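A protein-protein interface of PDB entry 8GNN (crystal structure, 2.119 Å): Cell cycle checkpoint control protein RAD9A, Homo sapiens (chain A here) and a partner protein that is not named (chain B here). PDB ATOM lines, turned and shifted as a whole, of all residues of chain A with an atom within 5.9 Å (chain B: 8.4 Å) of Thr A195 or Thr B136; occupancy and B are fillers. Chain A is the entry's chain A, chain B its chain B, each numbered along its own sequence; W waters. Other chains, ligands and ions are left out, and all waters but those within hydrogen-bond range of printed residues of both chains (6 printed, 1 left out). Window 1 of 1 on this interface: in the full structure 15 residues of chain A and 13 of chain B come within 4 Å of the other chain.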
ATOM      1  N   PRO A 158      -2.174 -23.881  14.068  1.00  0.00           N
ATOM      2  CA  PRO A 158      -3.567 -23.634  14.474  1.00  0.00           C
ATOM      3  C   PRO A 158      -3.988 -24.271  15.802  1.00  0.00           C
ATOM      4  O   PRO A 158      -4.972 -23.825  16.391  1.00  0.00           O
ATOM      5  CB  PRO A 158      -4.379 -24.245  13.326  1.00  0.00           C
ATOM      6  CG  PRO A 158      -3.461 -24.253  12.169  1.00  0.00           C
ATOM      7  CD  PRO A 158      -2.111 -24.526  12.742  1.00  0.00           C
ATOM      8  N   PHE A 159      -3.271 -25.292  16.261  1.00  0.00           N
ATOM      9  CA  PHE A 159      -3.660 -25.987  17.486  1.00  0.00           C
ATOM     10  C   PHE A 159      -3.351 -25.168  18.732  1.00  0.00           C
ATOM     11  O   PHE A 159      -2.522 -24.258  18.702  1.00  0.00           O
ATOM     12  CB  PHE A 159      -2.963 -27.345  17.582  1.00  0.00           C
ATOM     13  CG  PHE A 159      -3.284 -28.272  16.450  1.00  0.00           C
ATOM     14  CD1 PHE A 159      -4.538 -28.851  16.345  1.00  0.00           C
ATOM     15  CD2 PHE A 159      -2.329 -28.574  15.495  1.00  0.00           C
ATOM     16  CE1 PHE A 159      -4.835 -29.708  15.305  1.00  0.00           C
ATOM     17  CE2 PHE A 159      -2.620 -29.431  14.451  1.00  0.00           C
ATOM     18  CZ  PHE A 159      -3.875 -29.999  14.356  1.00  0.00           C
ATOM     19  N   LEU A 178      -3.865 -33.069   9.818  1.00  0.00           N
ATOM     20  CA  LEU A 178      -3.537 -32.998  11.235  1.00  0.00           C
ATOM     21  C   LEU A 178      -4.786 -32.636  12.026  1.00  0.00           C
ATOM     22  O   LEU A 178      -5.343 -31.552  11.854  1.00  0.00           O
ATOM     23  CB  LEU A 178      -2.425 -31.978  11.499  1.00  0.00           C
ATOM     24  CG  LEU A 178      -0.978 -32.477  11.484  1.00  0.00           C
ATOM     25  CD1 LEU A 178      -0.617 -33.096  10.144  1.00  0.00           C
ATOM     26  CD2 LEU A 178      -0.023 -31.344  11.828  1.00  0.00           C
ATOM     27  N   ARG A 179      -5.229 -33.548  12.882  1.00  0.00           N
ATOM     28  CA  ARG A 179      -6.427 -33.320  13.680  1.00  0.00           C
ATOM     29  C   ARG A 179      -6.131 -33.460  15.168  1.00  0.00           C
ATOM     30  O   ARG A 179      -5.467 -34.406  15.590  1.00  0.00           O
ATOM     31  CB  ARG A 179      -7.537 -34.291  13.270  1.00  0.00           C
ATOM     32  CG  ARG A 179      -8.833 -34.115  14.047  1.00  0.00           C
ATOM     33  CD  ARG A 179      -9.891 -35.120  13.614  1.00  0.00           C
ATOM     34  NE  ARG A 179     -10.124 -35.092  12.172  1.00  0.00           N
ATOM     35  CZ  ARG A 179      -9.766 -36.064  11.339  1.00  0.00           C
ATOM     36  NH1 ARG A 179      -9.158 -37.148  11.803  1.00  0.00           N
ATOM     37  NH2 ARG A 179     -10.016 -35.953  10.041  1.00  0.00           N
ATOM     38  N   SER A 180      -6.625 -32.510  15.955  1.00  0.00           N
ATOM     39  CA  SER A 180      -6.467 -32.563  17.403  1.00  0.00           C
ATOM     40  C   SER A 180      -7.155 -33.800  17.966  1.00  0.00           C
ATOM     41  O   SER A 180      -8.244 -34.167  17.529  1.00  0.00           O
ATOM     42  CB  SER A 180      -7.033 -31.300  18.056  1.00  0.00           C
ATOM     43  OG  SER A 180      -8.416 -31.158  17.782  1.00  0.00           O
ATOM     44  N   HIS A 182      -8.669 -35.855  21.383  1.00  0.00           N
ATOM     45  CA  HIS A 182      -9.241 -35.572  22.692  1.00  0.00           C
ATOM     46  C   HIS A 182      -9.817 -36.831  23.326  1.00  0.00           C
ATOM     47  O   HIS A 182     -10.582 -37.561  22.694  1.00  0.00           O
ATOM     48  CB  HIS A 182     -10.327 -34.500  22.580  1.00  0.00           C
ATOM     49  CG  HIS A 182      -9.872 -33.253  21.887  1.00  0.00           C
ATOM     50  ND1 HIS A 182      -9.142 -32.273  22.522  1.00  0.00           N
ATOM     51  CD2 HIS A 182     -10.036 -32.833  20.611  1.00  0.00           C
ATOM     52  CE1 HIS A 182      -8.879 -31.299  21.668  1.00  0.00           C
ATOM     53  NE2 HIS A 182      -9.411 -31.615  20.502  1.00  0.00           N
ATOM     54  N   MET A 193     -13.327 -28.282  21.401  1.00  0.00           N
ATOM     55  CA  MET A 193     -13.296 -27.856  20.008  1.00  0.00           C
ATOM     56  C   MET A 193     -12.287 -28.679  19.217  1.00  0.00           C
ATOM     57  O   MET A 193     -11.115 -28.756  19.581  1.00  0.00           O
ATOM     58  CB  MET A 193     -12.957 -26.367  19.898  1.00  0.00           C
ATOM     59  CG  MET A 193     -12.822 -25.876  18.461  1.00  0.00           C
ATOM     60  SD  MET A 193     -12.607 -24.091  18.322  1.00  0.00           S
ATOM     61  CE  MET A 193     -10.916 -23.898  18.872  1.00  0.00           C
ATOM     62  N   VAL A 194     -12.751 -29.298  18.137  1.00  0.00           N
ATOM     63  CA  VAL A 194     -11.874 -30.077  17.273  1.00  0.00           C
ATOM     64  C   VAL A 194     -11.267 -29.189  16.195  1.00  0.00           C
ATOM     65  O   VAL A 194     -11.980 -28.479  15.486  1.00  0.00           O
ATOM     66  CB  VAL A 194     -12.624 -31.250  16.611  1.00  0.00           C
ATOM     67  CG1 VAL A 194     -11.716 -31.974  15.627  1.00  0.00           C
ATOM     68  CG2 VAL A 194     -13.144 -32.210  17.668  1.00  0.00           C
ATOM     69  N   THR A 195      -9.943 -29.224  16.084  1.00  0.00           N
ATOM     70  CA  THR A 195      -9.243 -28.466  15.057  1.00  0.00           C
ATOM     71  C   THR A 195      -8.566 -29.406  14.070  1.00  0.00           C
ATOM     72  O   THR A 195      -7.881 -30.351  14.465  1.00  0.00           O
ATOM     73  CB  THR A 195      -8.192 -27.518  15.666  1.00  0.00           C
ATOM     74  OG1 THR A 195      -8.851 -26.506  16.437  1.00  0.00           O
ATOM     75  CG2 THR A 195      -7.368 -26.852  14.572  1.00  0.00           C
ATOM     76  N   GLU A 196      -8.772 -29.147  12.785  1.00  0.00           N
ATOM     77  CA  GLU A 196      -8.171 -29.958  11.737  1.00  0.00           C
ATOM     78  C   GLU A 196      -7.414 -29.093  10.737  1.00  0.00           C
ATOM     79  O   GLU A 196      -8.005 -28.255  10.058  1.00  0.00           O
ATOM     80  CB  GLU A 196      -9.244 -30.779  11.018  1.00  0.00           C
ATOM     81  CG  GLU A 196      -8.779 -31.403   9.714  1.00  0.00           C
ATOM     82  CD  GLU A 196      -9.837 -32.287   9.081  1.00  0.00           C
ATOM     83  OE1 GLU A 196     -10.340 -33.200   9.770  1.00  0.00           O
ATOM     84  OE2 GLU A 196     -10.168 -32.065   7.897  1.00  0.00           O
ATOM     85  N   MET A 197      -6.102 -29.287  10.664  1.00  0.00           N
ATOM     86  CA  MET A 197      -5.309 -28.663   9.614  1.00  0.00           C
ATOM     87  C   MET A 197      -5.189 -29.632   8.450  1.00  0.00           C
ATOM     88  O   MET A 197      -4.829 -30.796   8.630  1.00  0.00           O
ATOM     89  CB  MET A 197      -3.924 -28.256  10.117  1.00  0.00           C
ATOM     90  CG  MET A 197      -2.936 -27.966   8.994  1.00  0.00           C
ATOM     91  SD  MET A 197      -3.436 -26.596   7.926  1.00  0.00           S
ATOM     92  CE  MET A 197      -2.681 -25.208   8.767  1.00  0.00           C
ATOM     93  N   ASN B  93     -12.970 -20.469  22.410  1.00  0.00           N
ATOM     94  CA  ASN B  93     -13.041 -21.328  21.232  1.00  0.00           C
ATOM     95  C   ASN B  93     -13.199 -20.531  19.942  1.00  0.00           C
ATOM     96  O   ASN B  93     -12.531 -20.811  18.947  1.00  0.00           O
ATOM     97  CB  ASN B  93     -14.193 -22.326  21.369  1.00  0.00           C
ATOM     98  CG  ASN B  93     -13.876 -23.452  22.331  1.00  0.00           C
ATOM     99  OD1 ASN B  93     -12.812 -23.474  22.951  1.00  0.00           O
ATOM    100  ND2 ASN B  93     -14.802 -24.395  22.464  1.00  0.00           N
ATOM    101  N   ARG B  96      -9.890 -18.457  19.399  1.00  0.00           N
ATOM    102  CA  ARG B  96      -8.811 -19.307  18.907  1.00  0.00           C
ATOM    103  C   ARG B  96      -9.034 -19.664  17.442  1.00  0.00           C
ATOM    104  O   ARG B  96      -8.110 -19.614  16.630  1.00  0.00           O
ATOM    105  CB  ARG B  96      -8.703 -20.584  19.744  1.00  0.00           C
ATOM    106  CG  ARG B  96      -7.334 -21.245  19.690  1.00  0.00           C
ATOM    107  CD  ARG B  96      -7.423 -22.745  19.931  1.00  0.00           C
ATOM    108  NE  ARG B  96      -8.237 -23.080  21.095  1.00  0.00           N
ATOM    109  CZ  ARG B  96      -8.652 -24.309  21.385  1.00  0.00           C
ATOM    110  NH1 ARG B  96      -8.332 -25.322  20.593  1.00  0.00           N
ATOM    111  NH2 ARG B  96      -9.392 -24.525  22.464  1.00  0.00           N
ATOM    112  N   ALA B  97     -10.272 -20.019  17.116  1.00  0.00           N
ATOM    113  CA  ALA B  97     -10.643 -20.379  15.752  1.00  0.00           C
ATOM    114  C   ALA B  97     -10.437 -19.216  14.791  1.00  0.00           C
ATOM    115  O   ALA B  97      -9.971 -19.401  13.666  1.00  0.00           O
ATOM    116  CB  ALA B  97     -12.088 -20.848  15.708  1.00  0.00           C
ATOM    117  N   THR B 100      -6.836 -17.879  13.497  1.00  0.00           N
ATOM    118  CA  THR B 100      -6.384 -18.439  12.232  1.00  0.00           C
ATOM    119  C   THR B 100      -6.904 -17.582  11.083  1.00  0.00           C
ATOM    120  O   THR B 100      -6.233 -17.407  10.066  1.00  0.00           O
ATOM    121  CB  THR B 100      -6.865 -19.893  12.050  1.00  0.00           C
ATOM    122  OG1 THR B 100      -6.497 -20.670  13.198  1.00  0.00           O
ATOM    123  CG2 THR B 100      -6.250 -20.513  10.803  1.00  0.00           C
ATOM    124  N   LYS B 108     -15.184 -19.329   6.081  1.00  0.00           N
ATOM    125  CA  LYS B 108     -16.529 -19.884   6.024  1.00  0.00           C
ATOM    126  C   LYS B 108     -16.980 -20.302   7.414  1.00  0.00           C
ATOM    127  O   LYS B 108     -16.203 -20.857   8.191  1.00  0.00           O
ATOM    128  CB  LYS B 108     -16.594 -21.077   5.069  1.00  0.00           C
ATOM    129  CG  LYS B 108     -16.495 -20.713   3.598  1.00  0.00           C
ATOM    130  CD  LYS B 108     -16.640 -21.950   2.725  1.00  0.00           C
ATOM    131  CE  LYS B 108     -16.493 -21.612   1.252  1.00  0.00           C
ATOM    132  NZ  LYS B 108     -16.640 -22.819   0.394  1.00  0.00           N
ATOM    133  N   THR B 112     -23.319 -26.935  11.996  1.00  0.00           N
ATOM    134  CA  THR B 112     -23.241 -28.356  11.667  1.00  0.00           C
ATOM    135  C   THR B 112     -23.612 -29.248  12.847  1.00  0.00           C
ATOM    136  O   THR B 112     -23.740 -28.782  13.978  1.00  0.00           O
ATOM    137  CB  THR B 112     -21.830 -28.748  11.184  1.00  0.00           C
ATOM    138  OG1 THR B 112     -20.880 -28.507  12.230  1.00  0.00           O
ATOM    139  CG2 THR B 112     -21.440 -27.945   9.952  1.00  0.00           C
ATOM    140  N   LYS B 114     -22.159 -32.894  13.149  1.00  0.00           N
ATOM    141  CA  LYS B 114     -21.428 -34.122  12.857  1.00  0.00           C
ATOM    142  C   LYS B 114     -21.542 -35.106  14.016  1.00  0.00           C
ATOM    143  O   LYS B 114     -22.277 -36.091  13.937  1.00  0.00           O
ATOM    144  CB  LYS B 114     -19.957 -33.812  12.571  1.00  0.00           C
ATOM    145  CG  LYS B 114     -19.743 -32.698  11.558  1.00  0.00           C
ATOM    146  CD  LYS B 114     -18.337 -32.129  11.653  1.00  0.00           C
ATOM    147  CE  LYS B 114     -18.143 -30.966  10.693  1.00  0.00           C
ATOM    148  NZ  LYS B 114     -16.738 -30.471  10.698  1.00  0.00           N
ATOM    149  N   LEU B 119     -20.669 -24.907  15.775  1.00  0.00           N
ATOM    150  CA  LEU B 119     -20.478 -23.784  14.874  1.00  0.00           C
ATOM    151  C   LEU B 119     -19.147 -23.993  14.163  1.00  0.00           C
ATOM    152  O   LEU B 119     -18.086 -23.701  14.713  1.00  0.00           O
ATOM    153  CB  LEU B 119     -20.500 -22.457  15.632  1.00  0.00           C
ATOM    154  CG  LEU B 119     -20.538 -21.184  14.786  1.00  0.00           C
ATOM    155  CD1 LEU B 119     -21.758 -21.182  13.878  1.00  0.00           C
ATOM    156  CD2 LEU B 119     -20.528 -19.952  15.678  1.00  0.00           C
ATOM    157  N   THR B 120     -19.205 -24.524  12.947  1.00  0.00           N
ATOM    158  CA  THR B 120     -17.995 -24.914  12.236  1.00  0.00           C
ATOM    159  C   THR B 120     -17.359 -23.745  11.496  1.00  0.00           C
ATOM    160  O   THR B 120     -17.969 -23.141  10.614  1.00  0.00           O
ATOM    161  CB  THR B 120     -18.271 -26.048  11.235  1.00  0.00           C
ATOM    162  OG1 THR B 120     -18.661 -27.228  11.948  1.00  0.00           O
ATOM    163  CG2 THR B 120     -17.023 -26.350  10.420  1.00  0.00           C
ATOM    164  N   VAL B 121     -16.123 -23.436  11.871  1.00  0.00           N
ATOM    165  CA  VAL B 121     -15.362 -22.369  11.240  1.00  0.00           C
ATOM    166  C   VAL B 121     -14.315 -22.947  10.292  1.00  0.00           C
ATOM    167  O   VAL B 121     -13.352 -23.581  10.725  1.00  0.00           O
ATOM    168  CB  VAL B 121     -14.675 -21.478  12.295  1.00  0.00           C
ATOM    169  CG1 VAL B 121     -13.674 -20.544  11.643  1.00  0.00           C
ATOM    170  CG2 VAL B 121     -15.712 -20.690  13.078  1.00  0.00           C
ATOM    171  N   SER B 122     -14.518 -22.744   8.994  1.00  0.00           N
ATOM    172  CA  SER B 122     -13.552 -23.183   7.995  1.00  0.00           C
ATOM    173  C   SER B 122     -12.721 -22.001   7.518  1.00  0.00           C
ATOM    174  O   SER B 122     -13.262 -21.005   7.037  1.00  0.00           O
ATOM    175  CB  SER B 122     -14.251 -23.851   6.809  1.00  0.00           C
ATOM    176  OG  SER B 122     -14.852 -25.075   7.192  1.00  0.00           O
ATOM    177  N   VAL B 123     -11.405 -22.111   7.661  1.00  0.00           N
ATOM    178  CA  VAL B 123     -10.510 -21.034   7.266  1.00  0.00           C
ATOM    179  C   VAL B 123      -9.601 -21.466   6.125  1.00  0.00           C
ATOM    180  O   VAL B 123      -8.931 -22.497   6.203  1.00  0.00           O
ATOM    181  CB  VAL B 123      -9.649 -20.555   8.446  1.00  0.00           C
ATOM    182  CG1 VAL B 123      -8.802 -19.368   8.029  1.00  0.00           C
ATOM    183  CG2 VAL B 123     -10.529 -20.188   9.628  1.00  0.00           C
ATOM    184  N   GLU B 124      -9.589 -20.669   5.062  1.00  0.00           N
ATOM    185  CA  GLU B 124      -8.760 -20.948   3.898  1.00  0.00           C
ATOM    186  C   GLU B 124      -7.439 -20.192   3.978  1.00  0.00           C
ATOM    187  O   GLU B 124      -7.396 -18.979   3.776  1.00  0.00           O
ATOM    188  CB  GLU B 124      -9.503 -20.577   2.614  1.00  0.00           C
ATOM    189  CG  GLU B 124      -8.746 -20.883   1.335  1.00  0.00           C
ATOM    190  CD  GLU B 124      -9.576 -20.604   0.099  1.00  0.00           C
ATOM    191  OE1 GLU B 124     -10.727 -20.143   0.252  1.00  0.00           O
ATOM    192  OE2 GLU B 124      -9.079 -20.840  -1.023  1.00  0.00           O
ATOM    193  N   LEU B 125      -6.369 -20.913   4.296  1.00  0.00           N
ATOM    194  CA  LEU B 125      -5.033 -20.333   4.308  1.00  0.00           C
ATOM    195  C   LEU B 125      -4.363 -20.568   2.962  1.00  0.00           C
ATOM    196  O   LEU B 125      -4.656 -21.551   2.280  1.00  0.00           O
ATOM    197  CB  LEU B 125      -4.185 -20.927   5.434  1.00  0.00           C
ATOM    198  CG  LEU B 125      -4.749 -20.847   6.853  1.00  0.00           C
ATOM    199  CD1 LEU B 125      -3.789 -21.488   7.841  1.00  0.00           C
ATOM    200  CD2 LEU B 125      -5.039 -19.405   7.237  1.00  0.00           C
ATOM    201  N   ARG B 133      -4.386 -24.446   1.887  1.00  0.00           N
ATOM    202  CA  ARG B 133      -4.512 -25.113   3.176  1.00  0.00           C
ATOM    203  C   ARG B 133      -5.816 -24.734   3.863  1.00  0.00           C
ATOM    204  O   ARG B 133      -6.170 -23.558   3.939  1.00  0.00           O
ATOM    205  CB  ARG B 133      -3.323 -24.766   4.072  1.00  0.00           C
ATOM    206  CG  ARG B 133      -1.989 -25.216   3.513  1.00  0.00           C
ATOM    207  CD  ARG B 133      -0.837 -24.588   4.270  1.00  0.00           C
ATOM    208  NE  ARG B 133       0.453 -25.084   3.802  1.00  0.00           N
ATOM    209  CZ  ARG B 133       1.619 -24.537   4.125  1.00  0.00           C
ATOM    210  NH1 ARG B 133       1.655 -23.473   4.915  1.00  0.00           N
ATOM    211  NH2 ARG B 133       2.748 -25.050   3.656  1.00  0.00           N
ATOM    212  N   ILE B 134      -6.529 -25.739   4.363  1.00  0.00           N
ATOM    213  CA  ILE B 134      -7.810 -25.508   5.017  1.00  0.00           C
ATOM    214  C   ILE B 134      -7.773 -25.902   6.488  1.00  0.00           C
ATOM    215  O   ILE B 134      -7.465 -27.044   6.829  1.00  0.00           O
ATOM    216  CB  ILE B 134      -8.944 -26.289   4.324  1.00  0.00           C
ATOM    217  CG1 ILE B 134      -9.005 -25.937   2.837  1.00  0.00           C
ATOM    218  CG2 ILE B 134     -10.277 -26.007   5.001  1.00  0.00           C
ATOM    219  CD1 ILE B 134      -9.225 -24.465   2.567  1.00  0.00           C
ATOM    220  N   VAL B 135      -8.085 -24.945   7.355  1.00  0.00           N
ATOM    221  CA  VAL B 135      -8.212 -25.218   8.780  1.00  0.00           C
ATOM    222  C   VAL B 135      -9.683 -25.232   9.171  1.00  0.00           C
ATOM    223  O   VAL B 135     -10.416 -24.283   8.895  1.00  0.00           O
ATOM    224  CB  VAL B 135      -7.470 -24.177   9.635  1.00  0.00           C
ATOM    225  CG1 VAL B 135      -7.465 -24.603  11.093  1.00  0.00           C
ATOM    226  CG2 VAL B 135      -6.054 -24.000   9.134  1.00  0.00           C
ATOM    227  N   THR B 136     -10.112 -26.314   9.811  1.00  0.00           N
ATOM    228  CA  THR B 136     -11.501 -26.442  10.230  1.00  0.00           C
ATOM    229  C   THR B 136     -11.614 -26.518  11.748  1.00  0.00           C
ATOM    230  O   THR B 136     -11.061 -27.419  12.379  1.00  0.00           O
ATOM    231  CB  THR B 136     -12.165 -27.685   9.612  1.00  0.00           C
ATOM    232  OG1 THR B 136     -12.106 -27.600   8.183  1.00  0.00           O
ATOM    233  CG2 THR B 136     -13.618 -27.786  10.050  1.00  0.00           C
ATOM    234  N   HIS B 137     -12.328 -25.559  12.328  1.00  0.00           N
ATOM    235  CA  HIS B 137     -12.592 -25.560  13.760  1.00  0.00           C
ATOM    236  C   HIS B 137     -14.055 -25.880  14.027  1.00  0.00           C
ATOM    237  O   HIS B 137     -14.948 -25.180  13.550  1.00  0.00           O
ATOM    238  CB  HIS B 137     -12.239 -24.210  14.387  1.00  0.00           C
ATOM    239  CG  HIS B 137     -10.830 -23.769  14.137  1.00  0.00           C
ATOM    240  ND1 HIS B 137      -9.762 -24.231  14.875  1.00  0.00           N
ATOM    241  CD2 HIS B 137     -10.317 -22.892  13.241  1.00  0.00           C
ATOM    242  CE1 HIS B 137      -8.651 -23.664  14.439  1.00  0.00           C
ATOM    243  NE2 HIS B 137      -8.961 -22.848  13.449  1.00  0.00           N
ATOM    244  N   ASP B 138     -14.299 -26.939  14.789  1.00  0.00           N
ATOM    245  CA  ASP B 138     -15.656 -27.292  15.179  1.00  0.00           C
ATOM    246  C   ASP B 138     -15.949 -26.779  16.583  1.00  0.00           C
ATOM    247  O   ASP B 138     -15.626 -27.435  17.573  1.00  0.00           O
ATOM    248  CB  ASP B 138     -15.864 -28.806  15.104  1.00  0.00           C
ATOM    249  CG  ASP B 138     -15.715 -29.342  13.693  1.00  0.00           C
ATOM    250  OD1 ASP B 138     -16.197 -28.680  12.751  1.00  0.00           O
ATOM    251  OD2 ASP B 138     -15.112 -30.424  13.526  1.00  0.00           O
ATOM    252  N   ILE B 139     -16.552 -25.598  16.655  1.00  0.00           N
ATOM    253  CA  ILE B 139     -16.882 -24.972  17.929  1.00  0.00           C
ATOM    254  C   ILE B 139     -18.173 -25.541  18.499  1.00  0.00           C
ATOM    255  O   ILE B 139     -19.244 -25.333  17.932  1.00  0.00           O
ATOM    256  CB  ILE B 139     -17.035 -23.446  17.785  1.00  0.00           C
ATOM    257  CG1 ILE B 139     -15.774 -22.836  17.171  1.00  0.00           C
ATOM    258  CG2 ILE B 139     -17.346 -22.809  19.132  1.00  0.00           C
ATOM    259  CD1 ILE B 139     -15.935 -21.392  16.762  1.00  0.00           C
HETATM  260  O   HOH W   1      -9.658 -27.617  22.102  1.00  0.00           O
HETATM  261  O   HOH W   2      -8.734 -27.417  18.995  1.00  0.00           O
HETATM  262  O   HOH W   3      -9.697 -28.842   7.256  1.00  0.00           O
HETATM  263  O   HOH W   4     -15.918 -30.320  18.208  1.00  0.00           O
HETATM  264  O   HOH W   5      -7.094 -25.084  17.736  1.00  0.00           O
HETATM  265  O   HOH W   6     -11.918 -26.728  23.602  1.00  0.00           O
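The backbone carbonyl oxygen (O) of Val A194 is in hydrogen-bond range of the backbone NH (N) of Asp B138, 2.9 Å away. The backbone carbonyl oxygen (O) of Val A194 sits close to the backbone carbonyl oxygen (O) of Thr B136 (3.4 Å). A ring nitrogen (ND1) of His B137 lies within hydrogen-bond range of the side-chain hydroxyl (OG1) of Thr A195, 2.9 Å away. The backbone carbonyl oxygen (O) of Glu A196 sits at hydrogen-bond distance from the backbone NH (N) of Thr B136 (2.9 Å). The side-chain sulfur (SD) of Met A193 sits close to the backbone carbonyl oxygen (O) of Asn B93 (3.3 Å). O of Ile B134 sits close to O of Glu A196 (3.5 Å).
The backbone NH (N) of Ser A180 lies within hydrogen-bond range of the backbone carbonyl oxygen (O) of Thr A195. The backbone carbonyl oxygen (O) of Val B135 lies within hydrogen-bond range of the backbone NH (N) of Val B123 (2.7 Å). The backbone carbonyl oxygen (O) of Met A193 lies within hydrogen-bond range of a ring nitrogen (NE2) of His A182 (3.5 Å). OG1 of Thr B100 is in hydrogen-bond range of NE2 of His B137 (3.3 Å). N of Leu B119 lies within hydrogen-bond range of O of Ile B139, 2.6 Å away. The side-chain hydroxyl of Thr B120 lies within hydrogen-bond range of the side-chain carboxylate of Asp B138 (3.0 Å).
Pro A158 touches Val B135. Met A193 touches Arg B96. SD of Met A193 touches CB of His B137, 3.95 Å away. Met A193 touches Ile B139 (SD to CG1, 3.6 Å). His B137 touches Val A194 (CA to O, 3.4 Å). CA of Thr A195 touches O of Thr B136 (3.4 Å). Val B135 touches Glu A196 (CA to O, 3.3 Å). CE of Met A197 touches CD1 of Leu B125 (3.99 Å). Ile B134 touches Met A197. Val B135 touches Met A197 (CG2 to CE, 3.6 Å).
Printed residues of chain B within 4 Å of Thr A195: Thr B136 and His B137. Printed residues of chain B within 4 Å of Glu A196: Ile B134, Val B135 and Thr B136. Printed residues of chain A within 4 Å of Ile B139: Met A193. Of the printed residues of chain A, Asn B93 touches Met A193. The nearest residue of chain B that does not touch Thr A195 is Val B135 (4.1 Å). The nearest residue of chain A that does not touch Thr B136 is Met A197 (5.1 Å). The nearest printed residue of chain B that does not touch Val A194 is Ile B139 (5.5 Å).
Printed residues of chain A that touch a printed residue of chain B: Pro A158, Met A193, Val A194, Thr A195, Glu A196 and Met A197. Hydrophobic or aromatic side chains of chain A within 4 Å of the printed part of chain B: Pro A158, Met A193 and Met A197. Among the printed residues, 17 pairs touch across the chains. Among the printed residues, no Asp or Glu carboxylate lies within 4 Å of a Lys or Arg side-chain nitrogen of the other chain.
Water W5 lies within hydrogen-bond range of the side-chain hydroxyl (OG1) of Thr A195 (2.6 Å), the backbone carbonyl oxygen (O) of Pro A158 (2.8 Å) and the guanidinium group (NH1) of Arg B96 (3.1 Å). Water W2 lies within hydrogen-bond range of the guanidinium group of Arg B96, the side-chain hydroxyl of Thr A195 and the backbone carbonyl oxygen of Met A193. Water W3 lies within hydrogen-bond range of the side-chain hydroxyl (OG1) of Thr B136 (2.9 Å), the backbone carbonyl oxygen (O) of Ile B134 (2.9 Å) and the side-chain carboxylate (OE2) of Glu A196 (3.3 Å). Water W4 lies within hydrogen-bond range of O of Asp B138 (3.0 Å) and N of Val A194 (3.3 Å). Water W6 bridges the backbone NH (N) of Met A193 (3.0 Å) and the side-chain amide oxygen (OD1) of Asn B93 (3.4 Å). Water W1 lies within hydrogen-bond range of NH1 of Arg B96 (3.0 Å) and O of Met A193 (3.1 Å).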
